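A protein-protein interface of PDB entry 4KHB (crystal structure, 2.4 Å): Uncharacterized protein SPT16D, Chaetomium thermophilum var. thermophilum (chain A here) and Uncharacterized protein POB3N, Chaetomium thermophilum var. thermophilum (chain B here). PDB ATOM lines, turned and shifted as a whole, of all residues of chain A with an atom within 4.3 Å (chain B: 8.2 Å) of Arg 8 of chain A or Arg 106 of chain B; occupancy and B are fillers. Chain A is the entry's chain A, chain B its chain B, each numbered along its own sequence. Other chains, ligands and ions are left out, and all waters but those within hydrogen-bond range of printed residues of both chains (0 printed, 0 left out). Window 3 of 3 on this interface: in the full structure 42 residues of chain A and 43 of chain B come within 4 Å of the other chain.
Arg 8 of chain A touches one residue of chain B. Printed residues of chain A within 4 Å of Arg 106 of chain B: Arg 8 (3.2 Å), Glu 10 (3.6 Å) and Ser 11 (2.8 Å). Printed residues of chain A within 4 Å of Leu 105 of chain B: Ser 11 and Tyr 12. Of the printed residues of chain A, Trp 108 of chain B touches Phe 9. Of the printed residues of chain A, Trp 110 of chain B touches Phe 9. Of the printed residues of chain B, Phe 9 of chain A touches Trp 108 and Trp 110. Of the printed residues of chain A, Gly 107 of chain B touches Ser 11 (3.5 Å). Ser 104 of chain B touches none of the printed residues of chain A. Lys 7 of chain A touches none of the printed residues of chain B. The nearest printed residue of chain A that does not touch Arg 106 of chain B is Tyr 12 of chain A (4.01 Å). The nearest printed residue of chain A that does not touch Trp 110 of chain B is Lys 7 of chain A (6.3 Å).
Of the 13 printed residues of chain B, 5 touch a printed residue of chain A. Hydrophobic or aromatic side chains of chain B that line the printed part of chain A: Leu 105, Trp 108 and Trp 110. Along chain B the printed residues that touch a printed residue of chain A span positions 105 to 110. Of the 6 printed residues of chain A, 5 touch a printed residue of chain B. Among the printed residues, 8 pairs touch across the chains. Among the printed residues, no Asp or Glu carboxylate lies within 4 Å of a Lys or Arg side-chain nitrogen of the other chain.
O of Phe 9 of chain A sits at hydrogen-bond distance from NE1 of Trp 108 of chain B. The backbone NH (N) of Ser 11 of chain A lies within hydrogen-bond range of the backbone carbonyl oxygen (O) of Arg 106 of chain B, 2.8 Å away. The backbone NH of Tyr 12 of chain A sits at hydrogen-bond distance from the backbone carbonyl oxygen of Leu 105 of chain B (2.9 Å). The guanidinium group of Arg 106 of chain B sits close to the guanidinium group of Arg 8 of chain A, 3.2 Å away.
Phe 9 of chain A touches Trp 110 of chain B. Arg 106 of chain B touches Glu 10 of chain A (O to CA, 3.6 Å). Ser 11 of chain A touches Leu 105 of chain B. Gly 107 of chain B touches Ser 11 of chain A.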
ATOM      1  N   LYS A   7       6.025 -15.519  20.693  1.00  0.00           N
ATOM      2  CA  LYS A   7       7.477 -15.565  20.570  1.00  0.00           C
ATOM      3  C   LYS A   7       7.955 -14.749  19.379  1.00  0.00           C
ATOM      4  O   LYS A   7       8.582 -13.697  19.530  1.00  0.00           O
ATOM      5  CB  LYS A   7       7.946 -17.011  20.393  1.00  0.00           C
ATOM      6  CG  LYS A   7       9.433 -17.229  20.605  1.00  0.00           C
ATOM      7  CD  LYS A   7       9.731 -17.438  22.073  1.00  0.00           C
ATOM      8  CE  LYS A   7       9.063 -18.717  22.553  1.00  0.00           C
ATOM      9  NZ  LYS A   7       9.075 -18.864  24.031  1.00  0.00           N
ATOM     10  N   ARG A   8       7.643 -15.255  18.191  1.00  0.00           N
ATOM     11  CA  ARG A   8       8.069 -14.638  16.943  1.00  0.00           C
ATOM     12  C   ARG A   8       7.321 -13.347  16.627  1.00  0.00           C
ATOM     13  O   ARG A   8       6.086 -13.321  16.584  1.00  0.00           O
ATOM     14  CB  ARG A   8       7.904 -15.618  15.782  1.00  0.00           C
ATOM     15  CG  ARG A   8       8.318 -15.047  14.433  1.00  0.00           C
ATOM     16  CD  ARG A   8       8.460 -16.139  13.386  1.00  0.00           C
ATOM     17  NE  ARG A   8       8.887 -15.601  12.099  1.00  0.00           N
ATOM     18  CZ  ARG A   8      10.054 -15.887  11.531  1.00  0.00           C
ATOM     19  NH1 ARG A   8      10.896 -16.720  12.131  1.00  0.00           N
ATOM     20  NH2 ARG A   8      10.375 -15.358  10.361  1.00  0.00           N
ATOM     21  N   PHE A   9       8.081 -12.282  16.404  1.00  0.00           N
ATOM     22  CA  PHE A   9       7.524 -11.010  15.963  1.00  0.00           C
ATOM     23  C   PHE A   9       8.246 -10.560  14.700  1.00  0.00           C
ATOM     24  O   PHE A   9       9.272 -11.133  14.326  1.00  0.00           O
ATOM     25  CB  PHE A   9       7.617  -9.946  17.060  1.00  0.00           C
ATOM     26  CG  PHE A   9       8.992  -9.774  17.630  1.00  0.00           C
ATOM     27  CD1 PHE A   9       9.905  -8.913  17.037  1.00  0.00           C
ATOM     28  CD2 PHE A   9       9.364 -10.455  18.778  1.00  0.00           C
ATOM     29  CE1 PHE A   9      11.170  -8.748  17.570  1.00  0.00           C
ATOM     30  CE2 PHE A   9      10.624 -10.295  19.317  1.00  0.00           C
ATOM     31  CZ  PHE A   9      11.530  -9.438  18.712  1.00  0.00           C
ATOM     32  N   GLU A  10       7.708  -9.536  14.046  1.00  0.00           N
ATOM     33  CA  GLU A  10       8.238  -9.069  12.770  1.00  0.00           C
ATOM     34  C   GLU A  10       7.738  -7.657  12.500  1.00  0.00           C
ATOM     35  O   GLU A  10       6.528  -7.416  12.486  1.00  0.00           O
ATOM     36  CB  GLU A  10       7.775 -10.010  11.653  1.00  0.00           C
ATOM     37  CG  GLU A  10       7.788  -9.395  10.263  1.00  0.00           C
ATOM     38  CD  GLU A  10       7.227 -10.334   9.216  1.00  0.00           C
ATOM     39  OE1 GLU A  10       6.416  -9.874   8.388  1.00  0.00           O
ATOM     40  OE2 GLU A  10       7.587 -11.532   9.228  1.00  0.00           O
ATOM     41  N   SER A  11       8.664  -6.726  12.288  1.00  0.00           N
ATOM     42  CA  SER A  11       8.296  -5.333  12.076  1.00  0.00           C
ATOM     43  C   SER A  11       7.635  -5.147  10.714  1.00  0.00           C
ATOM     44  O   SER A  11       6.452  -4.815  10.628  1.00  0.00           O
ATOM     45  CB  SER A  11       9.521  -4.425  12.205  1.00  0.00           C
ATOM     46  OG  SER A  11      10.055  -4.465  13.518  1.00  0.00           O
ATOM     47  N   TYR A  12       8.407  -5.372   9.655  1.00  0.00           N
ATOM     48  CA  TYR A  12       7.913  -5.188   8.293  1.00  0.00           C
ATOM     49  C   TYR A  12       8.252  -6.385   7.405  1.00  0.00           C
ATOM     50  O   TYR A  12       9.168  -7.155   7.709  1.00  0.00           O
ATOM     51  CB  TYR A  12       8.503  -3.913   7.680  1.00  0.00           C
ATOM     52  CG  TYR A  12       8.217  -2.646   8.456  1.00  0.00           C
ATOM     53  CD1 TYR A  12       6.952  -2.071   8.450  1.00  0.00           C
ATOM     54  CD2 TYR A  12       9.217  -2.025   9.189  1.00  0.00           C
ATOM     55  CE1 TYR A  12       6.695  -0.911   9.157  1.00  0.00           C
ATOM     56  CE2 TYR A  12       8.971  -0.868   9.898  1.00  0.00           C
ATOM     57  CZ  TYR A  12       7.709  -0.317   9.878  1.00  0.00           C
ATOM     58  OH  TYR A  12       7.463   0.837  10.585  1.00  0.00           O
ATOM     59  N   HIS B 103      17.880  -6.104   2.378  1.00  0.00           N
ATOM     60  CA  HIS B 103      18.146  -5.927   3.797  1.00  0.00           C
ATOM     61  C   HIS B 103      17.009  -6.499   4.640  1.00  0.00           C
ATOM     62  O   HIS B 103      15.866  -6.583   4.178  1.00  0.00           O
ATOM     63  CB  HIS B 103      18.393  -4.452   4.114  1.00  0.00           C
ATOM     64  CG  HIS B 103      19.728  -3.954   3.651  1.00  0.00           C
ATOM     65  ND1 HIS B 103      20.064  -3.850   2.319  1.00  0.00           N
ATOM     66  CD2 HIS B 103      20.814  -3.545   4.347  1.00  0.00           C
ATOM     67  CE1 HIS B 103      21.299  -3.389   2.214  1.00  0.00           C
ATOM     68  NE2 HIS B 103      21.776  -3.195   3.430  1.00  0.00           N
ATOM     69  N   SER B 104      17.327  -6.886   5.873  1.00  0.00           N
ATOM     70  CA  SER B 104      16.341  -7.473   6.781  1.00  0.00           C
ATOM     71  C   SER B 104      15.375  -6.414   7.305  1.00  0.00           C
ATOM     72  O   SER B 104      15.791  -5.308   7.659  1.00  0.00           O
ATOM     73  CB  SER B 104      17.045  -8.176   7.948  1.00  0.00           C
ATOM     74  OG  SER B 104      16.104  -8.763   8.828  1.00  0.00           O
ATOM     75  N   LEU B 105      14.086  -6.745   7.342  1.00  0.00           N
ATOM     76  CA  LEU B 105      13.077  -5.789   7.791  1.00  0.00           C
ATOM     77  C   LEU B 105      12.278  -6.246   9.017  1.00  0.00           C
ATOM     78  O   LEU B 105      11.308  -5.588   9.400  1.00  0.00           O
ATOM     79  CB  LEU B 105      12.110  -5.481   6.641  1.00  0.00           C
ATOM     80  CG  LEU B 105      12.675  -4.757   5.413  1.00  0.00           C
ATOM     81  CD1 LEU B 105      11.612  -4.607   4.339  1.00  0.00           C
ATOM     82  CD2 LEU B 105      13.237  -3.402   5.796  1.00  0.00           C
ATOM     83  N   ARG B 106      12.675  -7.358   9.637  1.00  0.00           N
ATOM     84  CA  ARG B 106      11.913  -7.888  10.773  1.00  0.00           C
ATOM     85  C   ARG B 106      12.108  -7.097  12.070  1.00  0.00           C
ATOM     86  O   ARG B 106      11.292  -7.190  12.990  1.00  0.00           O
ATOM     87  CB  ARG B 106      12.082  -9.405  10.970  1.00  0.00           C
ATOM     88  CG  ARG B 106      13.490  -9.959  10.889  1.00  0.00           C
ATOM     89  CD  ARG B 106      13.520 -11.148   9.931  1.00  0.00           C
ATOM     90  NE  ARG B 106      13.948 -12.403  10.547  1.00  0.00           N
ATOM     91  CZ  ARG B 106      13.572 -13.607  10.120  1.00  0.00           C
ATOM     92  NH1 ARG B 106      12.761 -13.724   9.076  1.00  0.00           N
ATOM     93  NH2 ARG B 106      14.008 -14.698  10.732  1.00  0.00           N
ATOM     94  N   GLY B 107      13.193  -6.331  12.140  1.00  0.00           N
ATOM     95  CA  GLY B 107      13.444  -5.498  13.301  1.00  0.00           C
ATOM     96  C   GLY B 107      14.078  -6.225  14.468  1.00  0.00           C
ATOM     97  O   GLY B 107      13.905  -5.829  15.625  1.00  0.00           O
ATOM     98  N   TRP B 108      14.806  -7.297  14.170  1.00  0.00           N
ATOM     99  CA  TRP B 108      15.510  -8.047  15.203  1.00  0.00           C
ATOM    100  C   TRP B 108      16.822  -7.368  15.575  1.00  0.00           C
ATOM    101  O   TRP B 108      17.386  -6.603  14.783  1.00  0.00           O
ATOM    102  CB  TRP B 108      15.786  -9.475  14.735  1.00  0.00           C
ATOM    103  CG  TRP B 108      14.556 -10.324  14.619  1.00  0.00           C
ATOM    104  CD1 TRP B 108      13.262  -9.912  14.748  1.00  0.00           C
ATOM    105  CD2 TRP B 108      14.505 -11.731  14.347  1.00  0.00           C
ATOM    106  NE1 TRP B 108      12.409 -10.978  14.576  1.00  0.00           N
ATOM    107  CE2 TRP B 108      13.147 -12.105  14.328  1.00  0.00           C
ATOM    108  CE3 TRP B 108      15.477 -12.710  14.117  1.00  0.00           C
ATOM    109  CZ2 TRP B 108      12.737 -13.418  14.090  1.00  0.00           C
ATOM    110  CZ3 TRP B 108      15.068 -14.012  13.884  1.00  0.00           C
ATOM    111  CH2 TRP B 108      13.710 -14.353  13.872  1.00  0.00           C
ATOM    112  N   ASN B 109      17.304  -7.647  16.783  1.00  0.00           N
ATOM    113  CA  ASN B 109      18.577  -7.103  17.246  1.00  0.00           C
ATOM    114  C   ASN B 109      19.603  -8.194  17.538  1.00  0.00           C
ATOM    115  O   ASN B 109      20.617  -7.940  18.195  1.00  0.00           O
ATOM    116  CB  ASN B 109      18.382  -6.216  18.481  1.00  0.00           C
ATOM    117  CG  ASN B 109      18.040  -7.018  19.727  1.00  0.00           C
ATOM    118  OD1 ASN B 109      17.239  -7.953  19.677  1.00  0.00           O
ATOM    119  ND2 ASN B 109      18.648  -6.656  20.851  1.00  0.00           N
ATOM    120  N   TRP B 110      19.338  -9.405  17.053  1.00  0.00           N
ATOM    121  CA  TRP B 110      20.296 -10.499  17.209  1.00  0.00           C
ATOM    122  C   TRP B 110      20.674 -11.147  15.880  1.00  0.00           C
ATOM    123  O   TRP B 110      19.859 -11.213  14.953  1.00  0.00           O
ATOM    124  CB  TRP B 110      19.799 -11.552  18.209  1.00  0.00           C
ATOM    125  CG  TRP B 110      18.607 -12.348  17.770  1.00  0.00           C
ATOM    126  CD1 TRP B 110      18.619 -13.578  17.176  1.00  0.00           C
ATOM    127  CD2 TRP B 110      17.227 -12.000  17.929  1.00  0.00           C
ATOM    128  NE1 TRP B 110      17.334 -14.006  16.937  1.00  0.00           N
ATOM    129  CE2 TRP B 110      16.454 -13.046  17.398  1.00  0.00           C
ATOM    130  CE3 TRP B 110      16.563 -10.888  18.469  1.00  0.00           C
ATOM    131  CZ2 TRP B 110      15.061 -13.030  17.382  1.00  0.00           C
ATOM    132  CZ3 TRP B 110      15.179 -10.868  18.455  1.00  0.00           C
ATOM    133  CH2 TRP B 110      14.444 -11.928  17.914  1.00  0.00           C
ATOM    134  N   VAL B 124      21.116 -10.365   9.977  1.00  0.00           N
ATOM    135  CA  VAL B 124      20.006 -11.066  10.614  1.00  0.00           C
ATOM    136  C   VAL B 124      19.598 -12.226   9.717  1.00  0.00           C
ATOM    137  O   VAL B 124      18.999 -12.013   8.659  1.00  0.00           O
ATOM    138  CB  VAL B 124      18.800 -10.133  10.831  1.00  0.00           C
ATOM    139  CG1 VAL B 124      17.626 -10.899  11.422  1.00  0.00           C
ATOM    140  CG2 VAL B 124      19.182  -8.983  11.739  1.00  0.00           C
ATOM    141  N   GLN B 125      19.925 -13.445  10.144  1.00  0.00           N
ATOM    142  CA  GLN B 125      19.767 -14.642   9.314  1.00  0.00           C
ATOM    143  C   GLN B 125      20.360 -14.449   7.918  1.00  0.00           C
ATOM    144  O   GLN B 125      19.709 -14.724   6.905  1.00  0.00           O
ATOM    145  CB  GLN B 125      18.301 -15.081   9.239  1.00  0.00           C
ATOM    146  CG  GLN B 125      17.819 -15.765  10.516  1.00  0.00           C
ATOM    147  CD  GLN B 125      18.439 -17.139  10.708  1.00  0.00           C
ATOM    148  OE1 GLN B 125      18.648 -17.881   9.747  1.00  0.00           O
ATOM    149  NE2 GLN B 125      18.747 -17.479  11.954  1.00  0.00           N
ATOM    150  N   ASN B 126      21.594 -13.948   7.897  1.00  0.00           N
ATOM    151  CA  ASN B 126      22.391 -13.773   6.682  1.00  0.00           C
ATOM    152  C   ASN B 126      21.930 -12.655   5.739  1.00  0.00           C
ATOM    153  O   ASN B 126      22.353 -12.594   4.586  1.00  0.00           O
ATOM    154  CB  ASN B 126      22.579 -15.097   5.934  1.00  0.00           C
ATOM    155  CG  ASN B 126      23.773 -15.885   6.441  1.00  0.00           C
ATOM    156  OD1 ASN B 126      24.922 -15.510   6.205  1.00  0.00           O
ATOM    157  ND2 ASN B 126      23.508 -16.982   7.141  1.00  0.00           N
ATOM    158  N   ARG B 127      21.070 -11.771   6.238  1.00  0.00           N
ATOM    159  CA  ARG B 127      20.701 -10.568   5.501  1.00  0.00           C
ATOM    160  C   ARG B 127      21.017  -9.344   6.352  1.00  0.00           C
ATOM    161  O   ARG B 127      20.653  -9.284   7.528  1.00  0.00           O
ATOM    162  CB  ARG B 127      19.222 -10.597   5.096  1.00  0.00           C
ATOM    163  CG  ARG B 127      18.875 -11.718   4.125  1.00  0.00           C
ATOM    164  CD  ARG B 127      17.432 -11.654   3.653  1.00  0.00           C
ATOM    165  NE  ARG B 127      17.083 -12.815   2.838  1.00  0.00           N
ATOM    166  CZ  ARG B 127      15.847 -13.278   2.682  1.00  0.00           C
ATOM    167  NH1 ARG B 127      14.826 -12.679   3.280  1.00  0.00           N
ATOM    168  NH2 ARG B 127      15.629 -14.345   1.926  1.00  0.00           N
ATOM    169  N   ALA B 129      21.093  -5.969   8.285  1.00  0.00           N
ATOM    170  CA  ALA B 129      20.166  -4.996   8.843  1.00  0.00           C
ATOM    171  C   ALA B 129      20.746  -3.602   8.644  1.00  0.00           C
ATOM    172  O   ALA B 129      20.029  -2.663   8.285  1.00  0.00           O
ATOM    173  CB  ALA B 129      19.924  -5.267  10.320  1.00  0.00           C
